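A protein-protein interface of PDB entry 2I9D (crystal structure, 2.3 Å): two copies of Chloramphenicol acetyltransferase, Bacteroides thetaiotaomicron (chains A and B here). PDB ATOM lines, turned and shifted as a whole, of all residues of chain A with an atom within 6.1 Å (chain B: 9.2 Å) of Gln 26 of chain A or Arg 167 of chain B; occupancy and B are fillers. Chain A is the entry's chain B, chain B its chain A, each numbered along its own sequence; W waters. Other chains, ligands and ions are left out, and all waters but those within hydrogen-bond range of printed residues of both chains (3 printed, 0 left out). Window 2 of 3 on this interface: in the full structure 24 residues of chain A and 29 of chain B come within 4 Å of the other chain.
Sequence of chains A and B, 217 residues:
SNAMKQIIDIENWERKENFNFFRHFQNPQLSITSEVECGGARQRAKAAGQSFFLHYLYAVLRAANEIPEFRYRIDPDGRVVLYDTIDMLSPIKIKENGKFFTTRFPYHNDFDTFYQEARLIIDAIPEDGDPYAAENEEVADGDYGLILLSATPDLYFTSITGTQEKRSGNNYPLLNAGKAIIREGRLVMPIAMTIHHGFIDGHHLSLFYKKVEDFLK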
ATOM      1  N   PHE A  22      18.162 -10.638   1.521  1.00  0.00           N
ATOM      2  CA  PHE A  22      18.585  -9.519   2.358  1.00  0.00           C
ATOM      3  C   PHE A  22      20.087  -9.368   2.618  1.00  0.00           C
ATOM      4  O   PHE A  22      20.557  -8.272   2.905  1.00  0.00           O
ATOM      5  CB  PHE A  22      17.815  -9.556   3.659  1.00  0.00           C
ATOM      6  CG  PHE A  22      16.334  -9.331   3.475  1.00  0.00           C
ATOM      7  CD1 PHE A  22      15.833  -8.044   3.245  1.00  0.00           C
ATOM      8  CD2 PHE A  22      15.449 -10.411   3.482  1.00  0.00           C
ATOM      9  CE1 PHE A  22      14.484  -7.837   3.062  1.00  0.00           C
ATOM     10  CE2 PHE A  22      14.109 -10.213   3.305  1.00  0.00           C
ATOM     11  CZ  PHE A  22      13.625  -8.914   3.091  1.00  0.00           C
ATOM     12  N   HIS A  24      23.111  -9.157   1.227  1.00  0.00           N
ATOM     13  CA  HIS A  24      24.005  -8.149   0.613  1.00  0.00           C
ATOM     14  C   HIS A  24      23.498  -6.677   0.794  1.00  0.00           C
ATOM     15  O   HIS A  24      24.115  -5.737   0.294  1.00  0.00           O
ATOM     16  CB  HIS A  24      24.189  -8.479  -0.894  1.00  0.00           C
ATOM     17  CG  HIS A  24      22.969  -8.180  -1.740  1.00  0.00           C
ATOM     18  ND1 HIS A  24      22.845  -7.028  -2.497  1.00  0.00           N
ATOM     19  CD2 HIS A  24      21.809  -8.865  -1.918  1.00  0.00           C
ATOM     20  CE1 HIS A  24      21.679  -7.024  -3.124  1.00  0.00           C
ATOM     21  NE2 HIS A  24      21.033  -8.131  -2.795  1.00  0.00           N
ATOM     22  N   PHE A  25      22.362  -6.477   1.466  1.00  0.00           N
ATOM     23  CA  PHE A  25      21.761  -5.136   1.575  1.00  0.00           C
ATOM     24  C   PHE A  25      22.596  -4.187   2.448  1.00  0.00           C
ATOM     25  O   PHE A  25      23.175  -4.612   3.467  1.00  0.00           O
ATOM     26  CB  PHE A  25      20.374  -5.204   2.207  1.00  0.00           C
ATOM     27  CG  PHE A  25      19.275  -5.584   1.271  1.00  0.00           C
ATOM     28  CD1 PHE A  25      19.524  -6.287   0.078  1.00  0.00           C
ATOM     29  CD2 PHE A  25      17.954  -5.287   1.609  1.00  0.00           C
ATOM     30  CE1 PHE A  25      18.479  -6.665  -0.763  1.00  0.00           C
ATOM     31  CE2 PHE A  25      16.913  -5.659   0.756  1.00  0.00           C
ATOM     32  CZ  PHE A  25      17.190  -6.364  -0.424  1.00  0.00           C
ATOM     33  N   GLN A  26      22.632  -2.907   2.050  1.00  0.00           N
ATOM     34  CA  GLN A  26      23.206  -1.840   2.891  1.00  0.00           C
ATOM     35  C   GLN A  26      22.608  -1.853   4.316  1.00  0.00           C
ATOM     36  O   GLN A  26      23.345  -1.746   5.310  1.00  0.00           O
ATOM     37  CB  GLN A  26      23.043  -0.463   2.228  1.00  0.00           C
ATOM     38  CG  GLN A  26      23.779   0.647   3.005  1.00  0.00           C
ATOM     39  CD  GLN A  26      23.914   1.923   2.203  1.00  0.00           C
ATOM     40  OE1 GLN A  26      24.414   1.900   1.076  1.00  0.00           O
ATOM     41  NE2 GLN A  26      23.486   3.041   2.773  1.00  0.00           N
ATOM     42  N   ASN A  27      21.277  -2.035   4.390  1.00  0.00           N
ATOM     43  CA  ASN A  27      20.571  -2.204   5.646  1.00  0.00           C
ATOM     44  C   ASN A  27      19.581  -3.372   5.539  1.00  0.00           C
ATOM     45  O   ASN A  27      18.487  -3.217   5.007  1.00  0.00           O
ATOM     46  CB  ASN A  27      19.845  -0.892   6.061  1.00  0.00           C
ATOM     47  CG  ASN A  27      19.071  -1.029   7.381  1.00  0.00           C
ATOM     48  OD1 ASN A  27      19.313  -1.969   8.137  1.00  0.00           O
ATOM     49  ND2 ASN A  27      18.147  -0.081   7.669  1.00  0.00           N
ATOM     50  N   PRO A  28      19.971  -4.558   6.044  1.00  0.00           N
ATOM     51  CA  PRO A  28      19.091  -5.759   6.045  1.00  0.00           C
ATOM     52  C   PRO A  28      18.162  -5.812   7.291  1.00  0.00           C
ATOM     53  O   PRO A  28      17.412  -6.767   7.472  1.00  0.00           O
ATOM     54  CB  PRO A  28      20.109  -6.897   6.124  1.00  0.00           C
ATOM     55  CG  PRO A  28      21.211  -6.286   7.035  1.00  0.00           C
ATOM     56  CD  PRO A  28      21.292  -4.833   6.663  1.00  0.00           C
ATOM     57  N   GLN A 164      22.722   0.845  13.789  1.00  0.00           N
ATOM     58  CA  GLN A 164      23.251  -0.241  12.999  1.00  0.00           C
ATOM     59  C   GLN A 164      24.764  -0.181  13.014  1.00  0.00           C
ATOM     60  O   GLN A 164      25.367   0.726  12.442  1.00  0.00           O
ATOM     61  CB  GLN A 164      22.731  -0.171  11.560  1.00  0.00           C
ATOM     62  CG  GLN A 164      22.956  -1.460  10.744  1.00  0.00           C
ATOM     63  CD  GLN A 164      22.731  -1.224   9.276  1.00  0.00           C
ATOM     64  OE1 GLN A 164      22.025  -0.284   8.893  1.00  0.00           O
ATOM     65  NE2 GLN A 164      23.335  -2.046   8.441  1.00  0.00           N
ATOM     66  N   LYS A 166      27.223  -2.511  11.819  1.00  0.00           N
ATOM     67  CA  LYS A 166      27.882  -2.788  10.552  1.00  0.00           C
ATOM     68  C   LYS A 166      26.880  -3.062   9.453  1.00  0.00           C
ATOM     69  O   LYS A 166      25.680  -3.146   9.717  1.00  0.00           O
ATOM     70  CB  LYS A 166      28.900  -3.924  10.699  1.00  0.00           C
ATOM     71  CG  LYS A 166      28.432  -5.081  11.512  1.00  0.00           C
ATOM     72  CD  LYS A 166      29.614  -5.831  12.091  1.00  0.00           C
ATOM     73  CE  LYS A 166      29.148  -6.910  13.046  1.00  0.00           C
ATOM     74  NZ  LYS A 166      30.283  -7.231  13.983  1.00  0.00           N
ATOM     75  N   ARG A 167      27.375  -3.145   8.220  1.00  0.00           N
ATOM     76  CA  ARG A 167      26.550  -3.392   7.053  1.00  0.00           C
ATOM     77  C   ARG A 167      25.682  -4.637   7.249  1.00  0.00           C
ATOM     78  O   ARG A 167      24.510  -4.638   6.891  1.00  0.00           O
ATOM     79  CB  ARG A 167      27.421  -3.537   5.806  1.00  0.00           C
ATOM     80  CG  ARG A 167      26.661  -3.309   4.527  1.00  0.00           C
ATOM     81  CD  ARG A 167      27.399  -3.917   3.334  1.00  0.00           C
ATOM     82  NE  ARG A 167      26.547  -4.067   2.148  1.00  0.00           N
ATOM     83  CZ  ARG A 167      26.227  -3.077   1.311  1.00  0.00           C
ATOM     84  NH1 ARG A 167      26.654  -1.839   1.535  1.00  0.00           N
ATOM     85  NH2 ARG A 167      25.450  -3.317   0.251  1.00  0.00           N
ATOM     86  N   SER A 168      26.243  -5.685   7.838  1.00  0.00           N
ATOM     87  CA  SER A 168      25.487  -6.925   8.002  1.00  0.00           C
ATOM     88  C   SER A 168      24.457  -6.846   9.136  1.00  0.00           C
ATOM     89  O   SER A 168      23.664  -7.762   9.316  1.00  0.00           O
ATOM     90  CB  SER A 168      26.434  -8.128   8.156  1.00  0.00           C
ATOM     91  OG  SER A 168      27.210  -8.048   9.335  1.00  0.00           O
ATOM     92  N   PHE B  22      19.372  15.152  -1.766  1.00  0.00           N
ATOM     93  CA  PHE B  22      19.522  13.776  -1.234  1.00  0.00           C
ATOM     94  C   PHE B  22      20.417  12.835  -2.070  1.00  0.00           C
ATOM     95  O   PHE B  22      20.754  11.731  -1.608  1.00  0.00           O
ATOM     96  CB  PHE B  22      18.153  13.125  -0.984  1.00  0.00           C
ATOM     97  CG  PHE B  22      17.293  13.866   0.006  1.00  0.00           C
ATOM     98  CD1 PHE B  22      17.574  13.813   1.372  1.00  0.00           C
ATOM     99  CD2 PHE B  22      16.187  14.589  -0.426  1.00  0.00           C
ATOM    100  CE1 PHE B  22      16.770  14.462   2.300  1.00  0.00           C
ATOM    101  CE2 PHE B  22      15.373  15.267   0.489  1.00  0.00           C
ATOM    102  CZ  PHE B  22      15.670  15.195   1.865  1.00  0.00           C
ATOM    103  N   ARG B  23      20.808  13.285  -3.271  1.00  0.00           N
ATOM    104  CA  ARG B  23      21.630  12.504  -4.232  1.00  0.00           C
ATOM    105  C   ARG B  23      22.813  11.743  -3.650  1.00  0.00           C
ATOM    106  O   ARG B  23      23.053  10.614  -4.039  1.00  0.00           O
ATOM    107  CB  ARG B  23      22.131  13.371  -5.404  1.00  0.00           C
ATOM    108  CG  ARG B  23      22.551  12.538  -6.642  1.00  0.00           C
ATOM    109  CD  ARG B  23      23.141  13.389  -7.796  1.00  0.00           C
ATOM    110  NE  ARG B  23      22.113  14.129  -8.538  1.00  0.00           N
ATOM    111  CZ  ARG B  23      21.320  13.603  -9.479  1.00  0.00           C
ATOM    112  NH1 ARG B  23      21.409  12.308  -9.807  1.00  0.00           N
ATOM    113  NH2 ARG B  23      20.428  14.374 -10.099  1.00  0.00           N
ATOM    114  N   HIS B  24      23.552  12.340  -2.726  1.00  0.00           N
ATOM    115  CA  HIS B  24      24.749  11.674  -2.197  1.00  0.00           C
ATOM    116  C   HIS B  24      24.613  11.128  -0.778  1.00  0.00           C
ATOM    117  O   HIS B  24      25.585  10.654  -0.194  1.00  0.00           O
ATOM    118  CB  HIS B  24      25.945  12.617  -2.339  1.00  0.00           C
ATOM    119  CG  HIS B  24      26.148  13.081  -3.749  1.00  0.00           C
ATOM    120  ND1 HIS B  24      26.486  12.215  -4.775  1.00  0.00           N
ATOM    121  CD2 HIS B  24      26.006  14.304  -4.318  1.00  0.00           C
ATOM    122  CE1 HIS B  24      26.559  12.890  -5.910  1.00  0.00           C
ATOM    123  NE2 HIS B  24      26.273  14.159  -5.660  1.00  0.00           N
ATOM    124  N   PHE B  25      23.386  11.151  -0.258  1.00  0.00           N
ATOM    125  CA  PHE B  25      23.066  10.629   1.073  1.00  0.00           C
ATOM    126  C   PHE B  25      23.314   9.130   1.193  1.00  0.00           C
ATOM    127  O   PHE B  25      22.915   8.368   0.300  1.00  0.00           O
ATOM    128  CB  PHE B  25      21.592  10.921   1.392  1.00  0.00           C
ATOM    129  CG  PHE B  25      21.355  12.280   2.010  1.00  0.00           C
ATOM    130  CD1 PHE B  25      21.959  13.430   1.477  1.00  0.00           C
ATOM    131  CD2 PHE B  25      20.513  12.407   3.121  1.00  0.00           C
ATOM    132  CE1 PHE B  25      21.731  14.676   2.025  1.00  0.00           C
ATOM    133  CE2 PHE B  25      20.288  13.657   3.708  1.00  0.00           C
ATOM    134  CZ  PHE B  25      20.893  14.804   3.154  1.00  0.00           C
ATOM    135  N   GLN B  26      23.951   8.731   2.293  1.00  0.00           N
ATOM    136  CA  GLN B  26      23.988   7.341   2.731  1.00  0.00           C
ATOM    137  C   GLN B  26      22.585   6.669   2.786  1.00  0.00           C
ATOM    138  O   GLN B  26      22.381   5.550   2.294  1.00  0.00           O
ATOM    139  CB  GLN B  26      24.725   7.199   4.082  1.00  0.00           C
ATOM    140  CG  GLN B  26      24.693   5.744   4.647  1.00  0.00           C
ATOM    141  CD  GLN B  26      25.697   5.474   5.781  1.00  0.00           C
ATOM    142  OE1 GLN B  26      26.834   5.951   5.751  1.00  0.00           O
ATOM    143  NE2 GLN B  26      25.278   4.699   6.774  1.00  0.00           N
ATOM    144  N   ASN B  27      21.623   7.366   3.372  1.00  0.00           N
ATOM    145  CA  ASN B  27      20.261   6.898   3.420  1.00  0.00           C
ATOM    146  C   ASN B  27      19.322   8.058   3.092  1.00  0.00           C
ATOM    147  O   ASN B  27      19.084   8.908   3.941  1.00  0.00           O
ATOM    148  CB  ASN B  27      19.978   6.301   4.815  1.00  0.00           C
ATOM    149  CG  ASN B  27      18.530   6.045   5.047  1.00  0.00           C
ATOM    150  OD1 ASN B  27      17.747   5.962   4.102  1.00  0.00           O
ATOM    151  ND2 ASN B  27      18.147   5.949   6.296  1.00  0.00           N
ATOM    152  N   PRO B  28      18.821   8.119   1.839  1.00  0.00           N
ATOM    153  CA  PRO B  28      17.877   9.155   1.352  1.00  0.00           C
ATOM    154  C   PRO B  28      16.405   8.848   1.632  1.00  0.00           C
ATOM    155  O   PRO B  28      15.531   9.555   1.140  1.00  0.00           O
ATOM    156  CB  PRO B  28      18.087   9.113  -0.163  1.00  0.00           C
ATOM    157  CG  PRO B  28      18.346   7.661  -0.436  1.00  0.00           C
ATOM    158  CD  PRO B  28      19.179   7.172   0.756  1.00  0.00           C
ATOM    159  N   GLN B  29      16.142   7.814   2.427  1.00  0.00           N
ATOM    160  CA  GLN B  29      14.786   7.296   2.582  1.00  0.00           C
ATOM    161  C   GLN B  29      14.189   7.815   3.849  1.00  0.00           C
ATOM    162  O   GLN B  29      14.879   8.056   4.839  1.00  0.00           O
ATOM    163  CB  GLN B  29      14.789   5.770   2.671  1.00  0.00           C
ATOM    164  CG  GLN B  29      15.459   5.090   1.478  1.00  0.00           C
ATOM    165  CD  GLN B  29      15.271   3.600   1.463  1.00  0.00           C
ATOM    166  OE1 GLN B  29      15.036   3.020   0.412  1.00  0.00           O
ATOM    167  NE2 GLN B  29      15.373   2.965   2.633  1.00  0.00           N
ATOM    168  N   ILE B  74      14.039   5.741  -9.435  1.00  0.00           N
ATOM    169  CA  ILE B  74      15.378   5.803  -9.973  1.00  0.00           C
ATOM    170  C   ILE B  74      15.488   4.481 -10.715  1.00  0.00           C
ATOM    171  O   ILE B  74      15.496   3.403 -10.080  1.00  0.00           O
ATOM    172  CB  ILE B  74      16.476   5.897  -8.880  1.00  0.00           C
ATOM    173  CG1 ILE B  74      16.284   7.137  -7.986  1.00  0.00           C
ATOM    174  CG2 ILE B  74      17.880   5.864  -9.531  1.00  0.00           C
ATOM    175  CD1 ILE B  74      17.399   7.373  -6.942  1.00  0.00           C
ATOM    176  N   GLY B 162      11.608   0.392   6.926  1.00  0.00           N
ATOM    177  CA  GLY B 162      12.044  -0.466   5.858  1.00  0.00           C
ATOM    178  C   GLY B 162      13.532  -0.765   5.884  1.00  0.00           C
ATOM    179  O   GLY B 162      14.355  -0.013   6.473  1.00  0.00           O
ATOM    180  N   THR B 163      13.867  -1.889   5.243  1.00  0.00           N
ATOM    181  CA  THR B 163      15.234  -2.203   4.837  1.00  0.00           C
ATOM    182  C   THR B 163      15.730  -1.208   3.765  1.00  0.00           C
ATOM    183  O   THR B 163      14.967  -0.408   3.230  1.00  0.00           O
ATOM    184  CB  THR B 163      15.324  -3.665   4.302  1.00  0.00           C
ATOM    185  OG1 THR B 163      14.267  -3.895   3.379  1.00  0.00           O
ATOM    186  CG2 THR B 163      15.188  -4.651   5.426  1.00  0.00           C
ATOM    187  N   GLN B 164      17.013  -1.241   3.474  1.00  0.00           N
ATOM    188  CA  GLN B 164      17.542  -0.424   2.418  1.00  0.00           C
ATOM    189  C   GLN B 164      18.540  -1.282   1.588  1.00  0.00           C
ATOM    190  O   GLN B 164      19.584  -1.707   2.103  1.00  0.00           O
ATOM    191  CB  GLN B 164      18.207   0.831   3.020  1.00  0.00           C
ATOM    192  CG  GLN B 164      18.611   1.892   1.995  1.00  0.00           C
ATOM    193  CD  GLN B 164      19.621   2.904   2.570  1.00  0.00           C
ATOM    194  OE1 GLN B 164      19.739   3.076   3.801  1.00  0.00           O
ATOM    195  NE2 GLN B 164      20.365   3.560   1.681  1.00  0.00           N
ATOM    196  N   GLU B 165      18.220  -1.536   0.324  1.00  0.00           N
ATOM    197  CA  GLU B 165      19.079  -2.379  -0.492  1.00  0.00           C
ATOM    198  C   GLU B 165      20.454  -1.772  -0.808  1.00  0.00           C
ATOM    199  O   GLU B 165      21.501  -2.420  -0.652  1.00  0.00           O
ATOM    200  CB  GLU B 165      18.385  -2.799  -1.790  1.00  0.00           C
ATOM    201  CG  GLU B 165      19.358  -3.527  -2.746  1.00  0.00           C
ATOM    202  CD  GLU B 165      18.698  -4.141  -3.972  1.00  0.00           C
ATOM    203  OE1 GLU B 165      17.460  -4.031  -4.103  1.00  0.00           O
ATOM    204  OE2 GLU B 165      19.434  -4.755  -4.800  1.00  0.00           O
ATOM    205  N   LYS B 166      20.429  -0.526  -1.251  1.00  0.00           N
ATOM    206  CA  LYS B 166      21.583   0.157  -1.804  1.00  0.00           C
ATOM    207  C   LYS B 166      21.567   1.627  -1.377  1.00  0.00           C
ATOM    208  O   LYS B 166      20.591   2.094  -0.821  1.00  0.00           O
ATOM    209  CB  LYS B 166      21.605   0.022  -3.350  1.00  0.00           C
ATOM    210  CG  LYS B 166      20.369   0.508  -4.044  1.00  0.00           C
ATOM    211  CD  LYS B 166      20.347   0.100  -5.509  1.00  0.00           C
ATOM    212  CE  LYS B 166      19.497  -1.102  -5.713  1.00  0.00           C
ATOM    213  NZ  LYS B 166      19.189  -1.361  -7.153  1.00  0.00           N
ATOM    214  N   ARG B 167      22.672   2.321  -1.640  1.00  0.00           N
ATOM    215  CA  ARG B 167      22.848   3.723  -1.290  1.00  0.00           C
ATOM    216  C   ARG B 167      21.810   4.687  -1.862  1.00  0.00           C
ATOM    217  O   ARG B 167      21.359   5.588  -1.158  1.00  0.00           O
ATOM    218  CB  ARG B 167      24.270   4.180  -1.623  1.00  0.00           C
ATOM    219  CG  ARG B 167      24.722   5.339  -0.772  1.00  0.00           C
ATOM    220  CD  ARG B 167      25.958   6.011  -1.327  1.00  0.00           C
ATOM    221  NE  ARG B 167      26.257   7.239  -0.577  1.00  0.00           N
ATOM    222  CZ  ARG B 167      26.875   7.287   0.608  1.00  0.00           C
ATOM    223  NH1 ARG B 167      27.260   6.171   1.215  1.00  0.00           N
ATOM    224  NH2 ARG B 167      27.113   8.463   1.193  1.00  0.00           N
ATOM    225  N   SER B 168      21.419   4.497  -3.121  1.00  0.00           N
ATOM    226  CA  SER B 168      20.394   5.346  -3.747  1.00  0.00           C
ATOM    227  C   SER B 168      18.987   5.028  -3.238  1.00  0.00           C
ATOM    228  O   SER B 168      18.020   5.716  -3.601  1.00  0.00           O
ATOM    229  CB  SER B 168      20.439   5.198  -5.281  1.00  0.00           C
ATOM    230  OG  SER B 168      20.164   3.869  -5.694  1.00  0.00           O
ATOM    231  N   GLY B 169      18.876   3.982  -2.418  1.00  0.00           N
ATOM    232  CA  GLY B 169      17.605   3.583  -1.810  1.00  0.00           C
ATOM    233  C   GLY B 169      16.988   2.338  -2.441  1.00  0.00           C
ATOM    234  O   GLY B 169      17.485   1.840  -3.454  1.00  0.00           O
ATOM    235  N   ASN B 170      15.892   1.847  -1.885  1.00  0.00           N
ATOM    236  CA  ASN B 170      15.168   0.733  -2.510  1.00  0.00           C
ATOM    237  C   ASN B 170      14.683   1.072  -3.913  1.00  0.00           C
ATOM    238  O   ASN B 170      14.413   2.234  -4.204  1.00  0.00           O
ATOM    239  CB  ASN B 170      13.966   0.331  -1.650  1.00  0.00           C
ATOM    240  CG  ASN B 170      14.366  -0.090  -0.261  1.00  0.00           C
ATOM    241  OD1 ASN B 170      15.406  -0.689  -0.079  1.00  0.00           O
ATOM    242  ND2 ASN B 170      13.529   0.199   0.721  1.00  0.00           N
ATOM    243  N   ASN B 171      14.528   0.055  -4.763  1.00  0.00           N
ATOM    244  CA  ASN B 171      14.001   0.262  -6.127  1.00  0.00           C
ATOM    245  C   ASN B 171      12.590   0.855  -6.168  1.00  0.00           C
ATOM    246  O   ASN B 171      12.287   1.648  -7.060  1.00  0.00           O
ATOM    247  CB  ASN B 171      14.064  -1.031  -6.938  1.00  0.00           C
ATOM    248  CG  ASN B 171      15.471  -1.540  -7.078  1.00  0.00           C
ATOM    249  OD1 ASN B 171      16.402  -0.756  -7.257  1.00  0.00           O
ATOM    250  ND2 ASN B 171      15.649  -2.854  -6.956  1.00  0.00           N
ATOM    251  N   HIS B 196      11.585   7.389  -0.960  1.00  0.00           N
ATOM    252  CA  HIS B 196      12.812   8.151  -1.197  1.00  0.00           C
ATOM    253  C   HIS B 196      12.464   9.624  -0.981  1.00  0.00           C
ATOM    254  O   HIS B 196      11.567  10.131  -1.631  1.00  0.00           O
ATOM    255  CB  HIS B 196      13.289   7.926  -2.638  1.00  0.00           C
ATOM    256  CG  HIS B 196      14.676   8.404  -2.899  1.00  0.00           C
ATOM    257  ND1 HIS B 196      15.019   9.736  -2.886  1.00  0.00           N
ATOM    258  CD2 HIS B 196      15.804   7.726  -3.223  1.00  0.00           C
ATOM    259  CE1 HIS B 196      16.306   9.862  -3.146  1.00  0.00           C
ATOM    260  NE2 HIS B 196      16.799   8.658  -3.382  1.00  0.00           N
HETATM  261  O   HOH W   1      22.106   2.591   5.299  1.00  0.00           O
HETATM  262  O   HOH W   2      18.173   2.421   6.205  1.00  0.00           O
HETATM  263  O   HOH W   3      15.462  -0.412   9.022  1.00  0.00           O
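The backbone carbonyl oxygen of Gln 26 of chain B lies within hydrogen-bond range of the side-chain amide nitrogen of Gln 26 of chain A (2.8 Å). N of Gln 26 of chain A sits at hydrogen-bond distance from O of Gln 164 of chain B, 3.3 Å away. The backbone NH of Asn 27 of chain A lies within hydrogen-bond range of the backbone carbonyl oxygen of Gln 164 of chain B (2.9 Å). O of Glu 165 of chain B lies within hydrogen-bond range of N of Gln 26 of chain A, at 3.0 Å. The backbone NH (N) of Arg 167 of chain B sits at hydrogen-bond distance from the side-chain amide oxygen (OE1) of Gln 26 of chain A (3.3 Å).
Among the printed residues, merely in contact across the chains: Asn 27 of chain A with Thr 163 of chain B (3.3 Å), Phe 25 of chain A with Glu 165 of chain B (3.5 Å), Phe 25 of chain A with Gln 164 of chain B (3.6 Å), His 24 of chain A with Glu 165 of chain B (3.6 Å), Pro 28 of chain A with Thr 163 of chain B (3.7 Å), Gln 26 of chain A with Lys 166 of chain B (3.8 Å), Phe 22 of chain A with Thr 163 of chain B (3.96 Å) and Asn 27 of chain A with Gly 162 of chain B (3.98 Å).
Gln 26 of chain A touches just these residues of chain B: Gln 26 (2.8 Å), Gln 164 (3.3 Å), Glu 165 (3.0 Å), Lys 166 (3.8 Å) and Arg 167 (3.3 Å). Of chain A, only Gln 26 (3.3 Å) comes within 4 Å of Arg 167 of chain B. Of the printed residues of chain B, Phe 22 of chain A touches Thr 163. Of the printed residues of chain B, Pro 28 of chain A touches Thr 163. Arg 167 of chain A touches none of the printed residues of chain B.
Water W3 lies within hydrogen-bond range of O of Gly 162 of chain B (2.8 Å) and ND2 of Asn 27 of chain A (3.0 Å). Water W1 bridges OE1 of Gln 164 of chain B (2.8 Å) and NE2 of Gln 26 of chain A (2.9 Å). Water W2 bridges ND2 of Asn 27 of chain A (2.9 Å) and OE1 of Gln 164 of chain B (2.9 Å).
Gln 26 of chain B touches its own counterpart, Gln 26 of chain A. Gln 26 of chain A touches Gln 164 of chain B, but with the chains exchanged Gln 164 of chain A does not touch Gln 26 of chain B (6.3 Å). Gln 26 of chain A touches Arg 167 of chain B, but with the chains exchanged Arg 167 of chain A does not touch Gln 26 of chain B (8.2 Å). Asn 27 of chain A touches Gln 164 of chain B, but with the chains exchanged Gln 164 of chain A does not touch Asn 27 of chain B (7.8 Å).
The backbone carbonyl oxygen (O) of Gln 26 of chain B is in hydrogen-bond range of the side-chain amide nitrogen (NE2) of Gln 164 of chain B. The backbone carbonyl oxygen of Thr 163 of chain B sits at hydrogen-bond distance from the side-chain amide nitrogen of Gln 29 of chain B. ND2 of Asn 170 of chain B sits at hydrogen-bond distance from O of Thr 163 of chain B (3.0 Å). The backbone carbonyl oxygen of Lys 166 of chain B is in hydrogen-bond range of the side-chain amide nitrogen of Gln 164 of chain B. The backbone NH of Glu 165 of chain B lies within hydrogen-bond range of the side-chain amide oxygen of Asn 170 of chain B (3.0 Å). NZ of Lys 166 of chain B lies within hydrogen-bond range of OD1 of Asn 171 of chain B, 2.9 Å away.
Hydrophobic or aromatic side chains of chain A that line the printed part of chain B: Phe 22, His 24 and Phe 25. Printed residues of chain B that touch a printed residue of chain A: Gln 26, Gly 162, Thr 163, Gln 164, Glu 165, Lys 166 and Arg 167. Among the printed residues, no Asp or Glu carboxylate lies within 4 Å of a Lys or Arg side-chain nitrogen of the other chain.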
